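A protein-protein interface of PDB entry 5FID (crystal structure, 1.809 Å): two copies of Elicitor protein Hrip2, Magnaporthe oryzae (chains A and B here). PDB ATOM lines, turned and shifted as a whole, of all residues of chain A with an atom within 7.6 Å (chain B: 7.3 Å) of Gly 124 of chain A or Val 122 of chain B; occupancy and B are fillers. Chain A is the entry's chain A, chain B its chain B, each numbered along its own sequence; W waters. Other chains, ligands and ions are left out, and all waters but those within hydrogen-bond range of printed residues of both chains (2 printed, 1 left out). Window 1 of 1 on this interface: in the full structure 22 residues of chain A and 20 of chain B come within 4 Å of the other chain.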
ATOM      1  N   SER A  68      -7.753   7.678 -21.662  1.00  0.00           N
ATOM      2  CA  SER A  68      -6.701   8.378 -22.394  1.00  0.00           C
ATOM      3  C   SER A  68      -5.542   8.600 -21.427  1.00  0.00           C
ATOM      4  O   SER A  68      -5.674   8.332 -20.238  1.00  0.00           O
ATOM      5  CB  SER A  68      -7.218   9.701 -22.953  1.00  0.00           C
ATOM      6  OG  SER A  68      -7.380  10.662 -21.921  1.00  0.00           O
ATOM      7  N   PRO A  73       1.097  16.318 -16.362  1.00  0.00           N
ATOM      8  CA  PRO A  73       1.377  15.214 -15.439  1.00  0.00           C
ATOM      9  C   PRO A  73       1.204  13.842 -16.096  1.00  0.00           C
ATOM     10  O   PRO A  73       0.416  13.683 -17.038  1.00  0.00           O
ATOM     11  CB  PRO A  73       0.328  15.414 -14.350  1.00  0.00           C
ATOM     12  CG  PRO A  73      -0.846  15.999 -15.091  1.00  0.00           C
ATOM     13  CD  PRO A  73      -0.257  16.873 -16.174  1.00  0.00           C
ATOM     14  N   TYR A  75      -0.548  11.136 -16.019  1.00  0.00           N
ATOM     15  CA  TYR A  75      -1.797  10.558 -15.528  1.00  0.00           C
ATOM     16  C   TYR A  75      -2.511   9.775 -16.623  1.00  0.00           C
ATOM     17  O   TYR A  75      -2.406  10.104 -17.814  1.00  0.00           O
ATOM     18  CB  TYR A  75      -2.774  11.647 -15.084  1.00  0.00           C
ATOM     19  CG  TYR A  75      -2.397  12.439 -13.852  1.00  0.00           C
ATOM     20  CD1 TYR A  75      -1.409  11.999 -12.970  1.00  0.00           C
ATOM     21  CD2 TYR A  75      -3.065  13.619 -13.552  1.00  0.00           C
ATOM     22  CE1 TYR A  75      -1.095  12.739 -11.828  1.00  0.00           C
ATOM     23  CE2 TYR A  75      -2.752  14.366 -12.411  1.00  0.00           C
ATOM     24  CZ  TYR A  75      -1.770  13.913 -11.557  1.00  0.00           C
ATOM     25  OH  TYR A  75      -1.461  14.660 -10.435  1.00  0.00           O
ATOM     26  N   GLY A  76      -3.258   8.759 -16.205  1.00  0.00           N
ATOM     27  CA  GLY A  76      -4.176   8.065 -17.089  1.00  0.00           C
ATOM     28  C   GLY A  76      -5.573   8.480 -16.672  1.00  0.00           C
ATOM     29  O   GLY A  76      -5.819   8.664 -15.483  1.00  0.00           O
ATOM     30  N   TYR A  77      -6.479   8.638 -17.635  1.00  0.00           N
ATOM     31  CA  TYR A  77      -7.826   9.102 -17.345  1.00  0.00           C
ATOM     32  C   TYR A  77      -8.824   8.034 -17.778  1.00  0.00           C
ATOM     33  O   TYR A  77      -8.600   7.345 -18.766  1.00  0.00           O
ATOM     34  CB  TYR A  77      -8.084  10.424 -18.070  1.00  0.00           C
ATOM     35  CG  TYR A  77      -7.075  11.513 -17.726  1.00  0.00           C
ATOM     36  CD1 TYR A  77      -7.153  12.214 -16.527  1.00  0.00           C
ATOM     37  CD2 TYR A  77      -6.043  11.834 -18.594  1.00  0.00           C
ATOM     38  CE1 TYR A  77      -6.230  13.215 -16.214  1.00  0.00           C
ATOM     39  CE2 TYR A  77      -5.120  12.821 -18.281  1.00  0.00           C
ATOM     40  CZ  TYR A  77      -5.221  13.508 -17.098  1.00  0.00           C
ATOM     41  OH  TYR A  77      -4.301  14.492 -16.798  1.00  0.00           O
ATOM     42  N   TYR A  78      -9.913   7.884 -17.031  1.00  0.00           N
ATOM     43  CA  TYR A  78     -10.878   6.820 -17.295  1.00  0.00           C
ATOM     44  C   TYR A  78     -12.277   7.290 -16.921  1.00  0.00           C
ATOM     45  O   TYR A  78     -12.467   7.989 -15.924  1.00  0.00           O
ATOM     46  CB  TYR A  78     -10.522   5.540 -16.515  1.00  0.00           C
ATOM     47  CG  TYR A  78     -10.125   5.834 -15.091  1.00  0.00           C
ATOM     48  CD1 TYR A  78      -8.836   6.249 -14.789  1.00  0.00           C
ATOM     49  CD2 TYR A  78     -11.038   5.725 -14.055  1.00  0.00           C
ATOM     50  CE1 TYR A  78      -8.465   6.554 -13.495  1.00  0.00           C
ATOM     51  CE2 TYR A  78     -10.671   6.020 -12.758  1.00  0.00           C
ATOM     52  CZ  TYR A  78      -9.386   6.436 -12.486  1.00  0.00           C
ATOM     53  OH  TYR A  78      -9.017   6.748 -11.187  1.00  0.00           O
ATOM     54  N   PRO A  97      -8.768   1.751 -11.752  1.00  0.00           N
ATOM     55  CA  PRO A  97      -7.435   1.837 -12.346  1.00  0.00           C
ATOM     56  C   PRO A  97      -6.410   1.122 -11.480  1.00  0.00           C
ATOM     57  O   PRO A  97      -5.210   1.286 -11.707  1.00  0.00           O
ATOM     58  CB  PRO A  97      -7.145   3.336 -12.301  1.00  0.00           C
ATOM     59  CG  PRO A  97      -7.783   3.750 -10.993  1.00  0.00           C
ATOM     60  CD  PRO A  97      -9.060   2.921 -10.901  1.00  0.00           C
ATOM     61  N   GLY A 100      -5.117   3.249  -5.130  1.00  0.00           N
ATOM     62  CA  GLY A 100      -4.599   4.589  -4.907  1.00  0.00           C
ATOM     63  C   GLY A 100      -5.296   5.730  -5.637  1.00  0.00           C
ATOM     64  O   GLY A 100      -4.810   6.865  -5.603  1.00  0.00           O
ATOM     65  N   CYS A 101      -6.417   5.447  -6.296  1.00  0.00           N
ATOM     66  CA  CYS A 101      -7.125   6.468  -7.074  1.00  0.00           C
ATOM     67  C   CYS A 101      -8.632   6.262  -7.004  1.00  0.00           C
ATOM     68  O   CYS A 101      -9.090   5.151  -6.743  1.00  0.00           O
ATOM     69  CB  CYS A 101      -6.672   6.436  -8.536  1.00  0.00           C
ATOM     70  SG  CYS A 101      -4.904   6.727  -8.783  1.00  0.00           S
ATOM     71  N   GLN A 102      -9.399   7.319  -7.256  1.00  0.00           N
ATOM     72  CA  GLN A 102     -10.858   7.223  -7.233  1.00  0.00           C
ATOM     73  C   GLN A 102     -11.369   6.243  -8.300  1.00  0.00           C
ATOM     74  O   GLN A 102     -10.902   6.257  -9.445  1.00  0.00           O
ATOM     75  CB  GLN A 102     -11.507   8.608  -7.402  1.00  0.00           C
ATOM     76  CG  GLN A 102     -12.984   8.654  -6.994  1.00  0.00           C
ATOM     77  CD  GLN A 102     -13.426  10.011  -6.455  1.00  0.00           C
ATOM     78  OE1 GLN A 102     -12.603  10.875  -6.141  1.00  0.00           O
ATOM     79  NE2 GLN A 102     -14.740  10.203  -6.341  1.00  0.00           N
ATOM     80  N   LYS A 121     -18.321  12.409 -15.147  1.00  0.00           N
ATOM     81  CA  LYS A 121     -17.498  11.812 -14.112  1.00  0.00           C
ATOM     82  C   LYS A 121     -16.335  11.132 -14.797  1.00  0.00           C
ATOM     83  O   LYS A 121     -16.489  10.096 -15.438  1.00  0.00           O
ATOM     84  CB  LYS A 121     -18.322  10.853 -13.245  1.00  0.00           C
ATOM     85  CG  LYS A 121     -19.289  11.603 -12.322  1.00  0.00           C
ATOM     86  CD  LYS A 121     -20.043  10.680 -11.384  1.00  0.00           C
ATOM     87  CE  LYS A 121     -20.910  11.487 -10.414  1.00  0.00           C
ATOM     88  NZ  LYS A 121     -21.724  10.583  -9.535  1.00  0.00           N
ATOM     89  N   VAL A 122     -15.178  11.778 -14.704  1.00  0.00           N
ATOM     90  CA  VAL A 122     -13.961  11.315 -15.346  1.00  0.00           C
ATOM     91  C   VAL A 122     -12.894  11.425 -14.281  1.00  0.00           C
ATOM     92  O   VAL A 122     -12.829  12.439 -13.595  1.00  0.00           O
ATOM     93  CB  VAL A 122     -13.616  12.209 -16.566  1.00  0.00           C
ATOM     94  CG1 VAL A 122     -12.351  11.726 -17.273  1.00  0.00           C
ATOM     95  CG2 VAL A 122     -14.767  12.225 -17.548  1.00  0.00           C
ATOM     96  N   TYR A 123     -12.089  10.378 -14.106  1.00  0.00           N
ATOM     97  CA  TYR A 123     -11.060  10.389 -13.072  1.00  0.00           C
ATOM     98  C   TYR A 123      -9.663  10.194 -13.638  1.00  0.00           C
ATOM     99  O   TYR A 123      -9.493   9.524 -14.662  1.00  0.00           O
ATOM    100  CB  TYR A 123     -11.334   9.324 -12.006  1.00  0.00           C
ATOM    101  CG  TYR A 123     -12.679   9.464 -11.339  1.00  0.00           C
ATOM    102  CD1 TYR A 123     -12.997  10.590 -10.597  1.00  0.00           C
ATOM    103  CD2 TYR A 123     -13.624   8.465 -11.438  1.00  0.00           C
ATOM    104  CE1 TYR A 123     -14.233  10.717  -9.978  1.00  0.00           C
ATOM    105  CE2 TYR A 123     -14.860   8.585 -10.827  1.00  0.00           C
ATOM    106  CZ  TYR A 123     -15.156   9.713 -10.104  1.00  0.00           C
ATOM    107  OH  TYR A 123     -16.382   9.824  -9.495  1.00  0.00           O
ATOM    108  N   GLY A 124      -8.678  10.784 -12.959  1.00  0.00           N
ATOM    109  CA  GLY A 124      -7.273  10.617 -13.295  1.00  0.00           C
ATOM    110  C   GLY A 124      -6.495   9.855 -12.226  1.00  0.00           C
ATOM    111  O   GLY A 124      -6.858   9.860 -11.044  1.00  0.00           O
ATOM    112  N   CYS A 125      -5.410   9.206 -12.644  1.00  0.00           N
ATOM    113  CA  CYS A 125      -4.603   8.390 -11.753  1.00  0.00           C
ATOM    114  C   CYS A 125      -3.182   8.329 -12.316  1.00  0.00           C
ATOM    115  O   CYS A 125      -3.010   8.230 -13.530  1.00  0.00           O
ATOM    116  CB  CYS A 125      -5.207   6.980 -11.700  1.00  0.00           C
ATOM    117  SG  CYS A 125      -4.465   5.824 -10.544  1.00  0.00           S
ATOM    118  N   PRO A 126      -2.160   8.388 -11.441  1.00  0.00           N
ATOM    119  CA  PRO A 126      -0.762   8.284 -11.879  1.00  0.00           C
ATOM    120  C   PRO A 126      -0.475   7.024 -12.685  1.00  0.00           C
ATOM    121  O   PRO A 126      -0.910   5.927 -12.311  1.00  0.00           O
ATOM    122  CB  PRO A 126       0.002   8.205 -10.563  1.00  0.00           C
ATOM    123  CG  PRO A 126      -0.834   8.999  -9.609  1.00  0.00           C
ATOM    124  CD  PRO A 126      -2.266   8.705 -10.006  1.00  0.00           C
ATOM    125  N   LEU A 127       0.270   7.179 -13.774  1.00  0.00           N
ATOM    126  CA  LEU A 127       0.631   6.053 -14.630  1.00  0.00           C
ATOM    127  C   LEU A 127       1.717   5.220 -13.956  1.00  0.00           C
ATOM    128  O   LEU A 127       2.480   5.746 -13.135  1.00  0.00           O
ATOM    129  CB  LEU A 127       1.145   6.574 -15.978  1.00  0.00           C
ATOM    130  CG  LEU A 127       0.155   7.371 -16.823  1.00  0.00           C
ATOM    131  CD1 LEU A 127       0.830   7.928 -18.067  1.00  0.00           C
ATOM    132  CD2 LEU A 127      -1.022   6.473 -17.201  1.00  0.00           C
ATOM    133  N   ILE A 129      -1.399   2.463 -15.218  1.00  0.00           N
ATOM    134  CA  ILE A 129      -2.617   1.870 -14.695  1.00  0.00           C
ATOM    135  C   ILE A 129      -3.136   0.876 -15.715  1.00  0.00           C
ATOM    136  O   ILE A 129      -2.800   0.967 -16.897  1.00  0.00           O
ATOM    137  CB  ILE A 129      -3.709   2.928 -14.461  1.00  0.00           C
ATOM    138  CG1 ILE A 129      -4.064   3.637 -15.769  1.00  0.00           C
ATOM    139  CG2 ILE A 129      -3.255   3.948 -13.430  1.00  0.00           C
ATOM    140  CD1 ILE A 129      -5.244   4.617 -15.648  1.00  0.00           C
ATOM    141  N   TYR B  23       2.970  23.017 -16.025  1.00  0.00           N
ATOM    142  CA  TYR B  23       3.263  21.584 -16.031  1.00  0.00           C
ATOM    143  C   TYR B  23       4.381  21.196 -16.998  1.00  0.00           C
ATOM    144  O   TYR B  23       4.997  20.145 -16.840  1.00  0.00           O
ATOM    145  CB  TYR B  23       1.995  20.791 -16.341  1.00  0.00           C
ATOM    146  CG  TYR B  23       1.350  20.129 -15.138  1.00  0.00           C
ATOM    147  CD1 TYR B  23       2.080  19.307 -14.293  1.00  0.00           C
ATOM    148  CD2 TYR B  23       0.001  20.313 -14.865  1.00  0.00           C
ATOM    149  CE1 TYR B  23       1.480  18.682 -13.203  1.00  0.00           C
ATOM    150  CE2 TYR B  23      -0.608  19.697 -13.772  1.00  0.00           C
ATOM    151  CZ  TYR B  23       0.138  18.880 -12.953  1.00  0.00           C
ATOM    152  OH  TYR B  23      -0.454  18.265 -11.868  1.00  0.00           O
ATOM    153  N   GLY B  66      -4.371  22.008  -9.457  1.00  0.00           N
ATOM    154  CA  GLY B  66      -3.796  21.635 -10.734  1.00  0.00           C
ATOM    155  C   GLY B  66      -4.829  21.652 -11.839  1.00  0.00           C
ATOM    156  O   GLY B  66      -5.982  21.291 -11.623  1.00  0.00           O
ATOM    157  N   SER B  68      -4.932  20.433 -16.101  1.00  0.00           N
ATOM    158  CA  SER B  68      -4.168  19.785 -17.168  1.00  0.00           C
ATOM    159  C   SER B  68      -5.054  19.267 -18.293  1.00  0.00           C
ATOM    160  O   SER B  68      -6.281  19.397 -18.245  1.00  0.00           O
ATOM    161  CB  SER B  68      -3.323  18.638 -16.626  1.00  0.00           C
ATOM    162  OG  SER B  68      -4.130  17.664 -16.005  1.00  0.00           O
ATOM    163  N   GLY B  76     -10.655  18.944 -19.887  1.00  0.00           N
ATOM    164  CA  GLY B  76      -9.674  19.554 -19.003  1.00  0.00           C
ATOM    165  C   GLY B  76      -9.773  18.841 -17.665  1.00  0.00           C
ATOM    166  O   GLY B  76     -10.852  18.356 -17.305  1.00  0.00           O
ATOM    167  N   TYR B  77      -8.667  18.752 -16.932  1.00  0.00           N
ATOM    168  CA  TYR B  77      -8.650  17.982 -15.695  1.00  0.00           C
ATOM    169  C   TYR B  77      -8.116  18.814 -14.543  1.00  0.00           C
ATOM    170  O   TYR B  77      -7.119  19.526 -14.692  1.00  0.00           O
ATOM    171  CB  TYR B  77      -7.784  16.733 -15.867  1.00  0.00           C
ATOM    172  CG  TYR B  77      -8.180  15.874 -17.042  1.00  0.00           C
ATOM    173  CD1 TYR B  77      -7.595  16.060 -18.279  1.00  0.00           C
ATOM    174  CD2 TYR B  77      -9.139  14.879 -16.915  1.00  0.00           C
ATOM    175  CE1 TYR B  77      -7.952  15.274 -19.371  1.00  0.00           C
ATOM    176  CE2 TYR B  77      -9.496  14.076 -18.007  1.00  0.00           C
ATOM    177  CZ  TYR B  77      -8.897  14.288 -19.228  1.00  0.00           C
ATOM    178  OH  TYR B  77      -9.228  13.514 -20.323  1.00  0.00           O
ATOM    179  N   TYR B  78      -8.770  18.714 -13.387  1.00  0.00           N
ATOM    180  CA  TYR B  78      -8.462  19.603 -12.268  1.00  0.00           C
ATOM    181  C   TYR B  78      -8.336  18.815 -10.982  1.00  0.00           C
ATOM    182  O   TYR B  78      -8.990  17.780 -10.792  1.00  0.00           O
ATOM    183  CB  TYR B  78      -9.504  20.735 -12.135  1.00  0.00           C
ATOM    184  CG  TYR B  78     -10.913  20.214 -12.225  1.00  0.00           C
ATOM    185  CD1 TYR B  78     -11.468  19.896 -13.457  1.00  0.00           C
ATOM    186  CD2 TYR B  78     -11.676  19.997 -11.081  1.00  0.00           C
ATOM    187  CE1 TYR B  78     -12.731  19.389 -13.552  1.00  0.00           C
ATOM    188  CE2 TYR B  78     -12.950  19.487 -11.174  1.00  0.00           C
ATOM    189  CZ  TYR B  78     -13.466  19.184 -12.410  1.00  0.00           C
ATOM    190  OH  TYR B  78     -14.732  18.671 -12.522  1.00  0.00           O
ATOM    191  N   GLU B  79      -7.490  19.317 -10.092  1.00  0.00           N
ATOM    192  CA  GLU B  79      -7.100  18.561  -8.916  1.00  0.00           C
ATOM    193  C   GLU B  79      -6.884  19.518  -7.764  1.00  0.00           C
ATOM    194  O   GLU B  79      -6.146  20.504  -7.899  1.00  0.00           O
ATOM    195  CB  GLU B  79      -5.809  17.779  -9.200  1.00  0.00           C
ATOM    196  CG  GLU B  79      -5.241  17.020  -8.000  1.00  0.00           C
ATOM    197  CD  GLU B  79      -4.041  16.161  -8.362  1.00  0.00           C
ATOM    198  OE1 GLU B  79      -3.438  16.408  -9.432  1.00  0.00           O
ATOM    199  OE2 GLU B  79      -3.686  15.235  -7.584  1.00  0.00           O
ATOM    200  N   LEU B  80      -7.542  19.241  -6.642  1.00  0.00           N
ATOM    201  CA  LEU B  80      -7.326  20.009  -5.416  1.00  0.00           C
ATOM    202  C   LEU B  80      -6.509  19.121  -4.474  1.00  0.00           C
ATOM    203  O   LEU B  80      -7.039  18.163  -3.887  1.00  0.00           O
ATOM    204  CB  LEU B  80      -8.666  20.349  -4.766  1.00  0.00           C
ATOM    205  CG  LEU B  80      -8.590  21.262  -3.549  1.00  0.00           C
ATOM    206  CD1 LEU B  80      -8.058  22.635  -3.977  1.00  0.00           C
ATOM    207  CD2 LEU B  80      -9.955  21.392  -2.871  1.00  0.00           C
ATOM    208  N   GLN B 102     -17.924  17.462 -11.821  1.00  0.00           N
ATOM    209  CA  GLN B 102     -17.761  17.315 -10.373  1.00  0.00           C
ATOM    210  C   GLN B 102     -16.924  18.423  -9.749  1.00  0.00           C
ATOM    211  O   GLN B 102     -15.901  18.827 -10.304  1.00  0.00           O
ATOM    212  CB  GLN B 102     -17.118  15.974 -10.024  1.00  0.00           C
ATOM    213  CG  GLN B 102     -17.938  14.771 -10.407  1.00  0.00           C
ATOM    214  CD  GLN B 102     -17.553  13.551  -9.607  1.00  0.00           C
ATOM    215  OE1 GLN B 102     -16.685  12.769 -10.015  1.00  0.00           O
ATOM    216  NE2 GLN B 102     -18.188  13.383  -8.446  1.00  0.00           N
ATOM    217  N   PHE B 104     -14.880  19.973  -6.159  1.00  0.00           N
ATOM    218  CA  PHE B 104     -14.346  19.633  -4.856  1.00  0.00           C
ATOM    219  C   PHE B 104     -15.041  20.576  -3.890  1.00  0.00           C
ATOM    220  O   PHE B 104     -15.006  21.791  -4.071  1.00  0.00           O
ATOM    221  CB  PHE B 104     -12.842  19.899  -4.783  1.00  0.00           C
ATOM    222  CG  PHE B 104     -11.998  18.903  -5.535  1.00  0.00           C
ATOM    223  CD1 PHE B 104     -11.726  19.076  -6.886  1.00  0.00           C
ATOM    224  CD2 PHE B 104     -11.444  17.813  -4.877  1.00  0.00           C
ATOM    225  CE1 PHE B 104     -10.928  18.160  -7.577  1.00  0.00           C
ATOM    226  CE2 PHE B 104     -10.645  16.893  -5.564  1.00  0.00           C
ATOM    227  CZ  PHE B 104     -10.384  17.072  -6.908  1.00  0.00           C
ATOM    228  N   SER B 115      -7.288  15.460  -3.091  1.00  0.00           N
ATOM    229  CA  SER B 115      -6.403  14.519  -3.748  1.00  0.00           C
ATOM    230  C   SER B 115      -5.228  14.223  -2.817  1.00  0.00           C
ATOM    231  O   SER B 115      -4.596  15.143  -2.273  1.00  0.00           O
ATOM    232  CB  SER B 115      -5.885  15.103  -5.057  1.00  0.00           C
ATOM    233  OG  SER B 115      -5.227  14.106  -5.818  1.00  0.00           O
ATOM    234  N   MET B 119      -4.464   8.335  -2.642  1.00  0.00           N
ATOM    235  CA  MET B 119      -5.882   8.387  -2.976  1.00  0.00           C
ATOM    236  C   MET B 119      -6.102   9.619  -3.838  1.00  0.00           C
ATOM    237  O   MET B 119      -6.679  10.620  -3.400  1.00  0.00           O
ATOM    238  CB  MET B 119      -6.767   8.427  -1.724  1.00  0.00           C
ATOM    239  CG  MET B 119      -8.234   8.209  -2.039  1.00  0.00           C
ATOM    240  SD  MET B 119      -8.452   6.553  -3.069  1.00  0.00           S
ATOM    241  CE  MET B 119      -7.512   5.412  -1.789  1.00  0.00           C
ATOM    242  N   LYS B 120      -5.610   9.537  -5.069  1.00  0.00           N
ATOM    243  CA  LYS B 120      -5.593  10.672  -5.979  1.00  0.00           C
ATOM    244  C   LYS B 120      -6.994  10.973  -6.486  1.00  0.00           C
ATOM    245  O   LYS B 120      -7.780  10.059  -6.782  1.00  0.00           O
ATOM    246  CB  LYS B 120      -4.649  10.394  -7.152  1.00  0.00           C
ATOM    247  CG  LYS B 120      -3.195  10.237  -6.724  1.00  0.00           C
ATOM    248  CD  LYS B 120      -2.516  11.606  -6.516  1.00  0.00           C
ATOM    249  CE  LYS B 120      -2.208  12.250  -7.867  1.00  0.00           C
ATOM    250  NZ  LYS B 120      -1.521  13.568  -7.718  1.00  0.00           N
ATOM    251  N   LYS B 121      -7.305  12.262  -6.563  1.00  0.00           N
ATOM    252  CA  LYS B 121      -8.597  12.727  -7.059  1.00  0.00           C
ATOM    253  C   LYS B 121      -8.390  13.798  -8.106  1.00  0.00           C
ATOM    254  O   LYS B 121      -8.063  14.935  -7.795  1.00  0.00           O
ATOM    255  CB  LYS B 121      -9.466  13.239  -5.910  1.00  0.00           C
ATOM    256  CG  LYS B 121      -9.857  12.133  -4.948  1.00  0.00           C
ATOM    257  CD  LYS B 121     -10.523  12.672  -3.683  1.00  0.00           C
ATOM    258  CE  LYS B 121     -10.119  11.821  -2.493  1.00  0.00           C
ATOM    259  NZ  LYS B 121     -11.154  10.803  -2.229  1.00  0.00           N
ATOM    260  N   VAL B 122      -8.548  13.398  -9.357  1.00  0.00           N
ATOM    261  CA  VAL B 122      -8.361  14.285 -10.485  1.00  0.00           C
ATOM    262  C   VAL B 122      -9.621  14.128 -11.304  1.00  0.00           C
ATOM    263  O   VAL B 122      -9.960  13.016 -11.689  1.00  0.00           O
ATOM    264  CB  VAL B 122      -7.159  13.848 -11.324  1.00  0.00           C
ATOM    265  CG1 VAL B 122      -6.983  14.777 -12.511  1.00  0.00           C
ATOM    266  CG2 VAL B 122      -5.894  13.819 -10.457  1.00  0.00           C
ATOM    267  N   TYR B 123     -10.326  15.229 -11.547  1.00  0.00           N
ATOM    268  CA  TYR B 123     -11.639  15.158 -12.189  1.00  0.00           C
ATOM    269  C   TYR B 123     -11.555  15.746 -13.588  1.00  0.00           C
ATOM    270  O   TYR B 123     -10.817  16.709 -13.814  1.00  0.00           O
ATOM    271  CB  TYR B 123     -12.678  15.938 -11.374  1.00  0.00           C
ATOM    272  CG  TYR B 123     -12.870  15.442  -9.955  1.00  0.00           C
ATOM    273  CD1 TYR B 123     -12.519  14.153  -9.590  1.00  0.00           C
ATOM    274  CD2 TYR B 123     -13.416  16.264  -8.985  1.00  0.00           C
ATOM    275  CE1 TYR B 123     -12.700  13.699  -8.285  1.00  0.00           C
ATOM    276  CE2 TYR B 123     -13.599  15.819  -7.681  1.00  0.00           C
ATOM    277  CZ  TYR B 123     -13.236  14.540  -7.338  1.00  0.00           C
ATOM    278  OH  TYR B 123     -13.419  14.103  -6.035  1.00  0.00           O
ATOM    279  N   GLY B 124     -12.313  15.182 -14.525  1.00  0.00           N
ATOM    280  CA  GLY B 124     -12.327  15.689 -15.890  1.00  0.00           C
ATOM    281  C   GLY B 124     -13.619  16.405 -16.240  1.00  0.00           C
ATOM    282  O   GLY B 124     -14.654  16.142 -15.625  1.00  0.00           O
HETATM  283  O   HOH W   1     -15.372  13.436 -12.199  1.00  0.00           O
HETATM  284  O   HOH W   2      -8.888  10.360  -9.288  1.00  0.00           O
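Of the printed residues of chain B, Ser 68 of chain A touches Tyr 77.
Printed residues of chain B within 4 Å of Gln 102 of chain A: Lys 120 (3.2 Å), Lys 121 (3.2 Å) and Tyr 123 (3.3 Å).
Gly 124 of chain A touches just one residue of chain B: Val 122 (2.9 Å).
Of the printed residues of chain A, Tyr 23 of chain B touches Pro 73 (3.7 Å).
Val 122 of chain B touches just these residues of chain A: Tyr 75 (3.7 Å), Val 122 (3.5 Å), Tyr 123 (3.2 Å) and Gly 124 (2.9 Å).
Printed residues of chain A within 4 Å of Tyr 123 of chain B: Gln 102 (3.3 Å), Val 122 (3.3 Å) and Tyr 123 (3.7 Å).
The nearest residue of chain B that does not touch Gly 124 of chain A is Lys 120 of chain B (4.4 Å).
The nearest printed residue of chain A that does not touch Gln 102 of chain B is Gln 102 of chain A (4.9 Å).
OH of Tyr 77 of chain B touches OG of Ser 68 of chain A (3.8 Å).
Tyr 23 of chain B touches Pro 73 of chain A.
Ser 68 of chain B touches Pro 73 of chain A.
CG2 of Val 122 of chain B touches CE2 of Tyr 75 of chain A, 3.7 Å away.
CD1 of Tyr 77 of chain A touches CE2 of Tyr 77 of chain B, at 3.3 Å.
C of Cys 101 of chain A touches SD of Met 119 of chain B, 3.9 Å away.
Val 122 of chain A touches Tyr 77 of chain B (CG1 to CE2, 3.8 Å).
Tyr 123 of chain A touches Val 122 of chain B.
Tyr 123 of chain B touches Tyr 123 of chain A (CD1 to CD1, 3.7 Å).
CD of Pro 126 of chain A touches CG of Lys 120 of chain B (3.7 Å).
O of Val 122 of chain B is in hydrogen-bond range of N of Gly 124 of chain A.
The backbone NH (N) of Met 119 of chain B sits close to the backbone carbonyl oxygen (O) of Gly 100 of chain A (3.3 Å).
OH of Tyr 75 of chain A lies within hydrogen-bond range of OE1 of Glu 79 of chain B.
The side-chain hydroxyl (OH) of Tyr 123 of chain B is in hydrogen-bond range of the side-chain amide oxygen (OE1) of Gln 102 of chain A.
N of Gly 124 of chain B sits at hydrogen-bond distance from O of Val 122 of chain A.
N of Gln 102 of chain A is in hydrogen-bond range of O of Lys 120 of chain B (3.2 Å).
The backbone carbonyl oxygen of Gly 100 of chain A lies within hydrogen-bond range of the backbone NH of Lys 120 of chain B, at 2.8 Å.
O of Val 122 of chain B sits close to O of Val 122 of chain A (3.5 Å).
OH of Tyr 123 of chain A is in hydrogen-bond range of OE1 of Gln 102 of chain B (3.0 Å).
The side-chain hydroxyl of Tyr 77 of chain A sits at hydrogen-bond distance from the side-chain hydroxyl of Ser 68 of chain B.
NZ of Lys 120 of chain B lies within hydrogen-bond range of OH of Tyr 75 of chain A (2.9 Å).
Water W1 lies within hydrogen-bond range of OE1 of Gln 102 of chain B (2.6 Å) and N of Val 122 of chain A (3.0 Å).
Water W2 lies within hydrogen-bond range of the backbone carbonyl oxygen of Gly 124 of chain A (2.7 Å), the backbone carbonyl oxygen of Lys 120 of chain B (2.8 Å) and the backbone NH of Val 122 of chain B (3.1 Å).
Tyr 77 of chain B touches its own counterpart, Tyr 77 of chain A.
Val 122 of chain A touches Tyr 123 of chain B, and with the chains exchanged Tyr 123 of chain A touches Val 122 of chain B.
Val 122 of chain A touches Gly 124 of chain B, and with the chains exchanged Gly 124 of chain A touches Val 122 of chain B.
Tyr 123 of chain B touches its own counterpart, Tyr 123 of chain A.
Of the 17 printed residues of chain B, 11 touch a printed residue of chain A.
Hydrophobic or aromatic side chains of chain B that line the printed part of chain A: Tyr 23, Tyr 77, Met 119, Val 122 and Tyr 123.
Of the 18 printed residues of chain A, 12 touch a printed residue of chain B.
Printed residues of chain A that touch a printed residue of chain B: Ser 68, Pro 73, Tyr 75, Tyr 77, Gly 100, Cys 101, Gln 102, Lys 121, Val 122, Tyr 123, Gly 124 and Pro 126.
Among the printed residues, no Asp or Glu carboxylate lies within 4 Å of a Lys or Arg side-chain nitrogen of the other chain.
The backbone carbonyl oxygen (O) of Ser 68 of chain A sits at hydrogen-bond distance from the backbone NH (N) of Tyr 77 of chain A (2.7 Å).
The backbone NH (N) of Ser 68 of chain B sits at hydrogen-bond distance from the backbone carbonyl oxygen (O) of Tyr 77 of chain B.
OH of Tyr 78 of chain A lies within hydrogen-bond range of O of Gln 102 of chain A, at 2.6 Å.
The side-chain amino group (NZ) of Lys 120 of chain B lies within salt-bridge range of the side-chain carboxylate (OE2) of Glu 79 of chain B (2.7 Å).
N of Tyr 78 of chain B sits at hydrogen-bond distance from O of Tyr 123 of chain B, 2.9 Å away.
OE2 of Glu 79 of chain B lies within hydrogen-bond range of OG of Ser 115 of chain B.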
